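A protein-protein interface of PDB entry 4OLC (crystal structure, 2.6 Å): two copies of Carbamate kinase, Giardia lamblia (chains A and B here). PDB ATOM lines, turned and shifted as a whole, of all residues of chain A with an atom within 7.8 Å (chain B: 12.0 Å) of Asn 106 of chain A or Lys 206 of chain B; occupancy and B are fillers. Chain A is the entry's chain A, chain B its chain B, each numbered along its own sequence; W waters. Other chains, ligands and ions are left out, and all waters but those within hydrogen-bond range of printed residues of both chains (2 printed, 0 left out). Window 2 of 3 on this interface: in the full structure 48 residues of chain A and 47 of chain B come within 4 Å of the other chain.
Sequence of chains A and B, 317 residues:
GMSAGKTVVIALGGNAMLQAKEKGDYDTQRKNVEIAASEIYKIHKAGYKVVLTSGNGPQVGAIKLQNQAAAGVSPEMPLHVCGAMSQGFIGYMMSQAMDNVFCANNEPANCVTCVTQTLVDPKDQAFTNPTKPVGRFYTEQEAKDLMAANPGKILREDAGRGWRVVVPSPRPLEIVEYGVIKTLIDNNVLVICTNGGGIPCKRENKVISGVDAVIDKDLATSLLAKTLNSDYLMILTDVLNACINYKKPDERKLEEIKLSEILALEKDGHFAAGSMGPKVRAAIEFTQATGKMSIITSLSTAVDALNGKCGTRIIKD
N of Ile 208 of chain B lies within hydrogen-bond range of OD1 of Asn 100 of chain A (2.9 Å).
The side-chain carboxylate of Asp 99 of chain A sits at hydrogen-bond distance from the side-chain amide nitrogen of Gln 117 of chain B, 2.9 Å away.
The side-chain amide nitrogen (NE2) of Gln 96 of chain A sits at hydrogen-bond distance from the side-chain sulfur (SG) of Cys 201 of chain B (3.6 Å).
OE1 of Gln 96 of chain A sits close to O of Ile 208 of chain B (3.4 Å).
NE2 of Gln 96 of chain A is in hydrogen-bond range of OE1 of Gln 117 of chain B.
O of Ser 209 of chain B lies within hydrogen-bond range of N of Lys 202 of chain B, 2.9 Å away.
O of Gln 96 of chain A sits close to ND2 of Asn 100 of chain A, at 3.2 Å.
The backbone carbonyl oxygen (O) of Cys 201 of chain B lies within hydrogen-bond range of the backbone NH (N) of Val 120 of chain B (2.9 Å).
N of Val 176 of chain B lies within hydrogen-bond range of O of Gln 117 of chain B, 3.0 Å away.
Gln 96 of chain A touches Ser 209 of chain B (OE1 to CA, 3.8 Å).
Asp 99 of chain A touches Val 176 of chain B (OD1 to CG1, 3.98 Å).
OD1 of Asn 100 of chain A touches CA of Val 207 of chain B, at 3.7 Å.
Lys 206 of chain B touches Cys 103 of chain A.
Asn 106 of chain A touches Lys 206 of chain B.
Printed residues of chain B within 4 Å of Asp 99 of chain A: Gln 117 and Val 176.
Phe 102 of chain A touches none of the printed residues of chain B.
Cys 103 of chain A touches just one residue of chain B: Lys 206.
No residue of chain B comes within 4 Å of Ala 104 of chain A.
No residue of chain B comes within 4 Å of Asn 105 of chain A.
Of chain B, only Lys 206 comes within 4 Å of Asn 106 of chain A.
No residue of chain B comes within 4 Å of Glu 107 of chain A.
No residue of chain B comes within 4 Å of Pro 108 of chain A.
Of the printed residues of chain A, Cys 201 of chain B touches Gln 96.
Lys 206 of chain B touches two residues of chain A.
The nearest residue of chain A that does not touch Lys 206 of chain B is Asn 100 of chain A (4.3 Å).
The nearest printed residue of chain A that does not touch Ser 209 of chain B is Asn 100 of chain A (5.4 Å).
Of the 13 printed residues of chain A, 5 touch a printed residue of chain B.
Of the 16 printed residues of chain B, 7 touch a printed residue of chain A.
Hydrophobic or aromatic side chains of chain B that line the printed part of chain A: Val 176, Val 207 and Ile 208.
Among the printed residues, 10 pairs touch across the chains.
Among the printed residues, no Asp or Glu carboxylate lies within 4 Å of a Lys or Arg side-chain nitrogen of the other chain.
No position is printed for both chains.
Of the 10 pairs that touch across the chains among the printed residues, none has its exchanged pair printed and touching as well.
Water W2 bridges OD1 of Asp 99 of chain A (2.8 Å) and NE2 of Gln 117 of chain B (3.5 Å).
Water W1 bridges the backbone carbonyl oxygen of Ile 208 of chain B (3.3 Å) and the side-chain amide oxygen of Gln 96 of chain A (3.4 Å).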
ATOM      1  N   TYR A  41     -21.564  28.405  27.794  1.00  0.00           N
ATOM      2  CA  TYR A  41     -21.635  27.619  26.577  1.00  0.00           C
ATOM      3  C   TYR A  41     -23.046  27.520  25.986  1.00  0.00           C
ATOM      4  O   TYR A  41     -23.197  27.197  24.821  1.00  0.00           O
ATOM      5  CB  TYR A  41     -21.049  26.218  26.770  1.00  0.00           C
ATOM      6  CG  TYR A  41     -21.045  25.438  25.479  1.00  0.00           C
ATOM      7  CD1 TYR A  41     -20.030  25.618  24.552  1.00  0.00           C
ATOM      8  CD2 TYR A  41     -22.070  24.558  25.170  1.00  0.00           C
ATOM      9  CE1 TYR A  41     -20.027  24.929  23.347  1.00  0.00           C
ATOM     10  CE2 TYR A  41     -22.080  23.859  23.968  1.00  0.00           C
ATOM     11  CZ  TYR A  41     -21.055  24.048  23.054  1.00  0.00           C
ATOM     12  OH  TYR A  41     -21.045  23.364  21.843  1.00  0.00           O
ATOM     13  N   GLN A  96      -9.556  27.285  29.595  1.00  0.00           N
ATOM     14  CA  GLN A  96      -9.526  25.820  29.725  1.00  0.00           C
ATOM     15  C   GLN A  96     -10.897  25.194  29.992  1.00  0.00           C
ATOM     16  O   GLN A  96     -11.229  24.128  29.458  1.00  0.00           O
ATOM     17  CB  GLN A  96      -8.551  25.392  30.812  1.00  0.00           C
ATOM     18  CG  GLN A  96      -8.312  23.896  30.890  1.00  0.00           C
ATOM     19  CD  GLN A  96      -7.245  23.542  31.896  1.00  0.00           C
ATOM     20  OE1 GLN A  96      -7.538  23.176  33.032  1.00  0.00           O
ATOM     21  NE2 GLN A  96      -5.994  23.674  31.494  1.00  0.00           N
ATOM     22  N   ASP A  99     -12.695  25.582  26.588  1.00  0.00           N
ATOM     23  CA  ASP A  99     -12.249  24.529  25.696  1.00  0.00           C
ATOM     24  C   ASP A  99     -12.953  23.234  26.073  1.00  0.00           C
ATOM     25  O   ASP A  99     -13.460  22.535  25.208  1.00  0.00           O
ATOM     26  CB  ASP A  99     -10.725  24.351  25.759  1.00  0.00           C
ATOM     27  CG  ASP A  99      -9.965  25.596  25.315  1.00  0.00           C
ATOM     28  OD1 ASP A  99      -8.929  25.923  25.931  1.00  0.00           O
ATOM     29  OD2 ASP A  99     -10.407  26.246  24.353  1.00  0.00           O
ATOM     30  N   ASN A 100     -13.010  22.915  27.367  1.00  0.00           N
ATOM     31  CA  ASN A 100     -13.561  21.615  27.774  1.00  0.00           C
ATOM     32  C   ASN A 100     -15.059  21.463  27.486  1.00  0.00           C
ATOM     33  O   ASN A 100     -15.527  20.380  27.150  1.00  0.00           O
ATOM     34  CB  ASN A 100     -13.248  21.269  29.240  1.00  0.00           C
ATOM     35  CG  ASN A 100     -11.750  21.094  29.507  1.00  0.00           C
ATOM     36  OD1 ASN A 100     -10.971  20.848  28.589  1.00  0.00           O
ATOM     37  ND2 ASN A 100     -11.352  21.208  30.781  1.00  0.00           N
ATOM     38  N   VAL A 101     -15.816  22.541  27.628  1.00  0.00           N
ATOM     39  CA  VAL A 101     -17.237  22.472  27.333  1.00  0.00           C
ATOM     40  C   VAL A 101     -17.409  22.293  25.844  1.00  0.00           C
ATOM     41  O   VAL A 101     -18.160  21.423  25.411  1.00  0.00           O
ATOM     42  CB  VAL A 101     -17.998  23.725  27.762  1.00  0.00           C
ATOM     43  CG1 VAL A 101     -19.429  23.359  28.064  1.00  0.00           C
ATOM     44  CG2 VAL A 101     -17.350  24.323  28.976  1.00  0.00           C
ATOM     45  N   PHE A 102     -16.707  23.108  25.059  1.00  0.00           N
ATOM     46  CA  PHE A 102     -16.741  22.956  23.611  1.00  0.00           C
ATOM     47  C   PHE A 102     -16.500  21.503  23.202  1.00  0.00           C
ATOM     48  O   PHE A 102     -17.301  20.932  22.479  1.00  0.00           O
ATOM     49  CB  PHE A 102     -15.712  23.856  22.926  1.00  0.00           C
ATOM     50  CG  PHE A 102     -16.180  25.265  22.702  1.00  0.00           C
ATOM     51  CD1 PHE A 102     -16.685  26.014  23.743  1.00  0.00           C
ATOM     52  CD2 PHE A 102     -16.077  25.852  21.449  1.00  0.00           C
ATOM     53  CE1 PHE A 102     -17.105  27.320  23.540  1.00  0.00           C
ATOM     54  CE2 PHE A 102     -16.492  27.161  21.237  1.00  0.00           C
ATOM     55  CZ  PHE A 102     -17.012  27.900  22.292  1.00  0.00           C
ATOM     56  N   CYS A 103     -15.409  20.905  23.669  1.00  0.00           N
ATOM     57  CA  CYS A 103     -15.039  19.557  23.244  1.00  0.00           C
ATOM     58  C   CYS A 103     -16.003  18.506  23.783  1.00  0.00           C
ATOM     59  O   CYS A 103     -16.274  17.484  23.138  1.00  0.00           O
ATOM     60  CB  CYS A 103     -13.599  19.226  23.648  1.00  0.00           C
ATOM     61  SG  CYS A 103     -12.890  17.773  22.809  1.00  0.00           S
ATOM     62  N   ALA A 104     -16.528  18.765  24.967  1.00  0.00           N
ATOM     63  CA  ALA A 104     -17.542  17.895  25.545  1.00  0.00           C
ATOM     64  C   ALA A 104     -18.728  17.750  24.587  1.00  0.00           C
ATOM     65  O   ALA A 104     -19.372  16.696  24.535  1.00  0.00           O
ATOM     66  CB  ALA A 104     -18.006  18.453  26.877  1.00  0.00           C
ATOM     67  N   ASN A 105     -18.995  18.818  23.835  1.00  0.00           N
ATOM     68  CA  ASN A 105     -20.129  18.899  22.920  1.00  0.00           C
ATOM     69  C   ASN A 105     -19.687  18.843  21.480  1.00  0.00           C
ATOM     70  O   ASN A 105     -20.363  19.373  20.599  1.00  0.00           O
ATOM     71  CB  ASN A 105     -20.889  20.206  23.134  1.00  0.00           C
ATOM     72  CG  ASN A 105     -21.668  20.213  24.416  1.00  0.00           C
ATOM     73  OD1 ASN A 105     -22.900  20.210  24.400  1.00  0.00           O
ATOM     74  ND2 ASN A 105     -20.961  20.205  25.544  1.00  0.00           N
ATOM     75  N   ASN A 106     -18.528  18.235  21.252  1.00  0.00           N
ATOM     76  CA  ASN A 106     -18.036  17.982  19.901  1.00  0.00           C
ATOM     77  C   ASN A 106     -17.907  19.204  18.998  1.00  0.00           C
ATOM     78  O   ASN A 106     -18.090  19.126  17.786  1.00  0.00           O
ATOM     79  CB  ASN A 106     -18.875  16.905  19.222  1.00  0.00           C
ATOM     80  CG  ASN A 106     -18.113  15.611  19.063  1.00  0.00           C
ATOM     81  OD1 ASN A 106     -17.627  15.294  17.967  1.00  0.00           O
ATOM     82  ND2 ASN A 106     -17.976  14.861  20.167  1.00  0.00           N
ATOM     83  N   GLU A 107     -17.592  20.337  19.598  1.00  0.00           N
ATOM     84  CA  GLU A 107     -17.235  21.510  18.834  1.00  0.00           C
ATOM     85  C   GLU A 107     -15.736  21.720  19.069  1.00  0.00           C
ATOM     86  O   GLU A 107     -15.291  21.869  20.211  1.00  0.00           O
ATOM     87  CB  GLU A 107     -18.053  22.696  19.332  1.00  0.00           C
ATOM     88  CG  GLU A 107     -17.894  23.952  18.531  1.00  0.00           C
ATOM     89  CD  GLU A 107     -18.818  25.066  18.994  1.00  0.00           C
ATOM     90  OE1 GLU A 107     -18.582  26.226  18.602  1.00  0.00           O
ATOM     91  OE2 GLU A 107     -19.782  24.789  19.745  1.00  0.00           O
ATOM     92  N   PRO A 108     -14.925  21.681  18.008  1.00  0.00           N
ATOM     93  CA  PRO A 108     -13.528  21.895  18.379  1.00  0.00           C
ATOM     94  C   PRO A 108     -13.364  23.255  19.067  1.00  0.00           C
ATOM     95  O   PRO A 108     -14.126  24.189  18.797  1.00  0.00           O
ATOM     96  CB  PRO A 108     -12.800  21.868  17.028  1.00  0.00           C
ATOM     97  CG  PRO A 108     -13.850  22.205  16.013  1.00  0.00           C
ATOM     98  CD  PRO A 108     -15.113  21.597  16.549  1.00  0.00           C
ATOM     99  N   ALA A 109     -12.378  23.357  19.952  1.00  0.00           N
ATOM    100  CA  ALA A 109     -12.140  24.585  20.697  1.00  0.00           C
ATOM    101  C   ALA A 109     -11.916  25.786  19.778  1.00  0.00           C
ATOM    102  O   ALA A 109     -11.372  25.651  18.680  1.00  0.00           O
ATOM    103  CB  ALA A 109     -10.954  24.399  21.639  1.00  0.00           C
ATOM    104  N   GLN B 117      -1.982  27.410  26.272  1.00  0.00           N
ATOM    105  CA  GLN B 117      -1.825  26.061  26.767  1.00  0.00           C
ATOM    106  C   GLN B 117      -1.102  25.213  25.726  1.00  0.00           C
ATOM    107  O   GLN B 117      -1.259  25.417  24.520  1.00  0.00           O
ATOM    108  CB  GLN B 117      -3.193  25.464  27.054  1.00  0.00           C
ATOM    109  CG  GLN B 117      -4.032  26.298  27.997  1.00  0.00           C
ATOM    110  CD  GLN B 117      -5.472  25.857  28.017  1.00  0.00           C
ATOM    111  OE1 GLN B 117      -5.895  25.093  28.890  1.00  0.00           O
ATOM    112  NE2 GLN B 117      -6.242  26.333  27.043  1.00  0.00           N
ATOM    113  N   LEU B 119      -0.248  21.094  24.990  1.00  0.00           N
ATOM    114  CA  LEU B 119      -0.454  19.718  25.411  1.00  0.00           C
ATOM    115  C   LEU B 119       0.853  18.963  25.394  1.00  0.00           C
ATOM    116  O   LEU B 119       1.730  19.261  24.594  1.00  0.00           O
ATOM    117  CB  LEU B 119      -1.484  19.016  24.550  1.00  0.00           C
ATOM    118  CG  LEU B 119      -2.843  19.709  24.568  1.00  0.00           C
ATOM    119  CD1 LEU B 119      -3.830  18.989  23.648  1.00  0.00           C
ATOM    120  CD2 LEU B 119      -3.373  19.811  26.004  1.00  0.00           C
ATOM    121  N   VAL B 120       0.985  18.028  26.327  1.00  0.00           N
ATOM    122  CA  VAL B 120       2.143  17.148  26.435  1.00  0.00           C
ATOM    123  C   VAL B 120       1.668  15.761  26.850  1.00  0.00           C
ATOM    124  O   VAL B 120       0.528  15.590  27.273  1.00  0.00           O
ATOM    125  CB  VAL B 120       3.161  17.645  27.489  1.00  0.00           C
ATOM    126  CG1 VAL B 120       3.610  19.083  27.192  1.00  0.00           C
ATOM    127  CG2 VAL B 120       2.586  17.524  28.892  1.00  0.00           C
ATOM    128  N   PRO B 122       1.497  12.876  29.381  1.00  0.00           N
ATOM    129  CA  PRO B 122       1.648  12.756  30.838  1.00  0.00           C
ATOM    130  C   PRO B 122       2.596  11.622  31.224  1.00  0.00           C
ATOM    131  O   PRO B 122       3.118  11.598  32.348  1.00  0.00           O
ATOM    132  CB  PRO B 122       0.229  12.420  31.317  1.00  0.00           C
ATOM    133  CG  PRO B 122      -0.666  12.649  30.147  1.00  0.00           C
ATOM    134  CD  PRO B 122       0.171  12.429  28.932  1.00  0.00           C
ATOM    135  N   GLU B 174       1.126  19.859  21.166  1.00  0.00           N
ATOM    136  CA  GLU B 174       0.140  20.683  20.490  1.00  0.00           C
ATOM    137  C   GLU B 174      -0.077  22.008  21.210  1.00  0.00           C
ATOM    138  O   GLU B 174      -0.284  22.037  22.416  1.00  0.00           O
ATOM    139  CB  GLU B 174      -1.182  19.916  20.348  1.00  0.00           C
ATOM    140  CG  GLU B 174      -2.379  20.765  19.905  1.00  0.00           C
ATOM    141  CD  GLU B 174      -3.642  19.922  19.614  1.00  0.00           C
ATOM    142  OE1 GLU B 174      -4.736  20.521  19.433  1.00  0.00           O
ATOM    143  OE2 GLU B 174      -3.539  18.668  19.560  1.00  0.00           O
ATOM    144  N   VAL B 176      -2.617  24.429  21.997  1.00  0.00           N
ATOM    145  CA  VAL B 176      -4.080  24.430  22.014  1.00  0.00           C
ATOM    146  C   VAL B 176      -4.690  25.605  21.267  1.00  0.00           C
ATOM    147  O   VAL B 176      -5.657  25.445  20.526  1.00  0.00           O
ATOM    148  CB  VAL B 176      -4.622  24.434  23.455  1.00  0.00           C
ATOM    149  CG1 VAL B 176      -6.108  24.608  23.446  1.00  0.00           C
ATOM    150  CG2 VAL B 176      -4.215  23.140  24.209  1.00  0.00           C
ATOM    151  N   CYS B 201      -0.196  20.994  29.814  1.00  0.00           N
ATOM    152  CA  CYS B 201      -1.451  20.323  30.138  1.00  0.00           C
ATOM    153  C   CYS B 201      -1.466  18.969  29.476  1.00  0.00           C
ATOM    154  O   CYS B 201      -0.599  18.661  28.668  1.00  0.00           O
ATOM    155  CB  CYS B 201      -2.668  21.125  29.668  1.00  0.00           C
ATOM    156  SG  CYS B 201      -2.766  22.849  30.253  1.00  0.00           S
ATOM    157  N   LYS B 202      -2.452  18.159  29.832  1.00  0.00           N
ATOM    158  CA  LYS B 202      -2.692  16.893  29.156  1.00  0.00           C
ATOM    159  C   LYS B 202      -4.152  16.843  28.717  1.00  0.00           C
ATOM    160  O   LYS B 202      -5.011  17.511  29.305  1.00  0.00           O
ATOM    161  CB  LYS B 202      -2.386  15.718  30.090  1.00  0.00           C
ATOM    162  CG  LYS B 202      -3.359  15.576  31.239  1.00  0.00           C
ATOM    163  CD  LYS B 202      -2.973  14.454  32.169  1.00  0.00           C
ATOM    164  CE  LYS B 202      -4.195  13.952  32.948  1.00  0.00           C
ATOM    165  NZ  LYS B 202      -4.112  14.196  34.415  1.00  0.00           N
ATOM    166  N   ARG B 203      -4.428  16.072  27.670  1.00  0.00           N
ATOM    167  CA  ARG B 203      -5.797  15.833  27.244  1.00  0.00           C
ATOM    168  C   ARG B 203      -6.095  14.344  27.326  1.00  0.00           C
ATOM    169  O   ARG B 203      -5.376  13.516  26.780  1.00  0.00           O
ATOM    170  CB  ARG B 203      -6.038  16.356  25.830  1.00  0.00           C
ATOM    171  CG  ARG B 203      -7.523  16.434  25.474  1.00  0.00           C
ATOM    172  CD  ARG B 203      -7.757  16.329  23.981  1.00  0.00           C
ATOM    173  NE  ARG B 203      -7.784  17.629  23.316  1.00  0.00           N
ATOM    174  CZ  ARG B 203      -7.056  17.924  22.246  1.00  0.00           C
ATOM    175  NH1 ARG B 203      -6.238  17.014  21.734  1.00  0.00           N
ATOM    176  NH2 ARG B 203      -7.142  19.128  21.700  1.00  0.00           N
ATOM    177  N   GLU B 204      -7.168  14.022  28.025  1.00  0.00           N
ATOM    178  CA  GLU B 204      -7.463  12.665  28.459  1.00  0.00           C
ATOM    179  C   GLU B 204      -8.958  12.460  28.322  1.00  0.00           C
ATOM    180  O   GLU B 204      -9.728  12.760  29.247  1.00  0.00           O
ATOM    181  CB  GLU B 204      -7.047  12.465  29.935  1.00  0.00           C
ATOM    182  CG  GLU B 204      -5.635  11.897  30.165  1.00  0.00           C
ATOM    183  CD  GLU B 204      -5.370  11.509  31.615  1.00  0.00           C
ATOM    184  OE1 GLU B 204      -4.281  10.961  31.910  1.00  0.00           O
ATOM    185  OE2 GLU B 204      -6.249  11.762  32.466  1.00  0.00           O
ATOM    186  N   ASN B 205      -9.361  11.950  27.166  1.00  0.00           N
ATOM    187  CA  ASN B 205     -10.772  11.816  26.832  1.00  0.00           C
ATOM    188  C   ASN B 205     -11.491  13.162  26.812  1.00  0.00           C
ATOM    189  O   ASN B 205     -12.383  13.409  27.621  1.00  0.00           O
ATOM    190  CB  ASN B 205     -11.477  10.842  27.784  1.00  0.00           C
ATOM    191  CG  ASN B 205     -12.901  10.529  27.348  1.00  0.00           C
ATOM    192  OD1 ASN B 205     -13.124   9.696  26.465  1.00  0.00           O
ATOM    193  ND2 ASN B 205     -13.871  11.196  27.966  1.00  0.00           N
ATOM    194  N   LYS B 206     -11.080  14.043  25.905  1.00  0.00           N
ATOM    195  CA  LYS B 206     -11.798  15.294  25.676  1.00  0.00           C
ATOM    196  C   LYS B 206     -11.778  16.326  26.822  1.00  0.00           C
ATOM    197  O   LYS B 206     -12.547  17.295  26.799  1.00  0.00           O
ATOM    198  CB  LYS B 206     -13.241  14.973  25.256  1.00  0.00           C
ATOM    199  CG  LYS B 206     -13.329  13.756  24.324  1.00  0.00           C
ATOM    200  CD  LYS B 206     -14.759  13.420  23.900  1.00  0.00           C
ATOM    201  CE  LYS B 206     -15.212  14.307  22.749  1.00  0.00           C
ATOM    202  NZ  LYS B 206     -14.221  14.328  21.624  1.00  0.00           N
ATOM    203  N   VAL B 207     -10.916  16.124  27.820  1.00  0.00           N
ATOM    204  CA  VAL B 207     -10.696  17.162  28.835  1.00  0.00           C
ATOM    205  C   VAL B 207      -9.216  17.511  29.094  1.00  0.00           C
ATOM    206  O   VAL B 207      -8.375  16.646  29.354  1.00  0.00           O
ATOM    207  CB  VAL B 207     -11.481  16.904  30.167  1.00  0.00           C
ATOM    208  CG1 VAL B 207     -11.852  15.428  30.331  1.00  0.00           C
ATOM    209  CG2 VAL B 207     -10.712  17.439  31.380  1.00  0.00           C
ATOM    210  N   ILE B 208      -8.926  18.805  28.992  1.00  0.00           N
ATOM    211  CA  ILE B 208      -7.600  19.358  29.211  1.00  0.00           C
ATOM    212  C   ILE B 208      -7.422  19.726  30.686  1.00  0.00           C
ATOM    213  O   ILE B 208      -8.297  20.346  31.284  1.00  0.00           O
ATOM    214  CB  ILE B 208      -7.410  20.636  28.349  1.00  0.00           C
ATOM    215  CG1 ILE B 208      -7.715  20.346  26.877  1.00  0.00           C
ATOM    216  CG2 ILE B 208      -6.004  21.233  28.523  1.00  0.00           C
ATOM    217  CD1 ILE B 208      -7.671  21.584  25.970  1.00  0.00           C
ATOM    218  N   SER B 209      -6.297  19.351  31.282  1.00  0.00           N
ATOM    219  CA  SER B 209      -6.012  19.745  32.666  1.00  0.00           C
ATOM    220  C   SER B 209      -4.520  19.974  32.841  1.00  0.00           C
ATOM    221  O   SER B 209      -3.698  19.364  32.147  1.00  0.00           O
ATOM    222  CB  SER B 209      -6.521  18.700  33.663  1.00  0.00           C
ATOM    223  OG  SER B 209      -5.889  17.452  33.455  1.00  0.00           O
ATOM    224  N   GLY B 210      -4.174  20.875  33.748  1.00  0.00           N
ATOM    225  CA  GLY B 210      -2.794  21.286  33.903  1.00  0.00           C
ATOM    226  C   GLY B 210      -1.934  20.280  34.645  1.00  0.00           C
ATOM    227  O   GLY B 210      -2.311  19.771  35.701  1.00  0.00           O
HETATM  228  O   HOH W   1      -9.254  20.617  34.480  1.00  0.00           O
HETATM  229  O   HOH W   2      -7.960  28.284  24.761  1.00  0.00           O
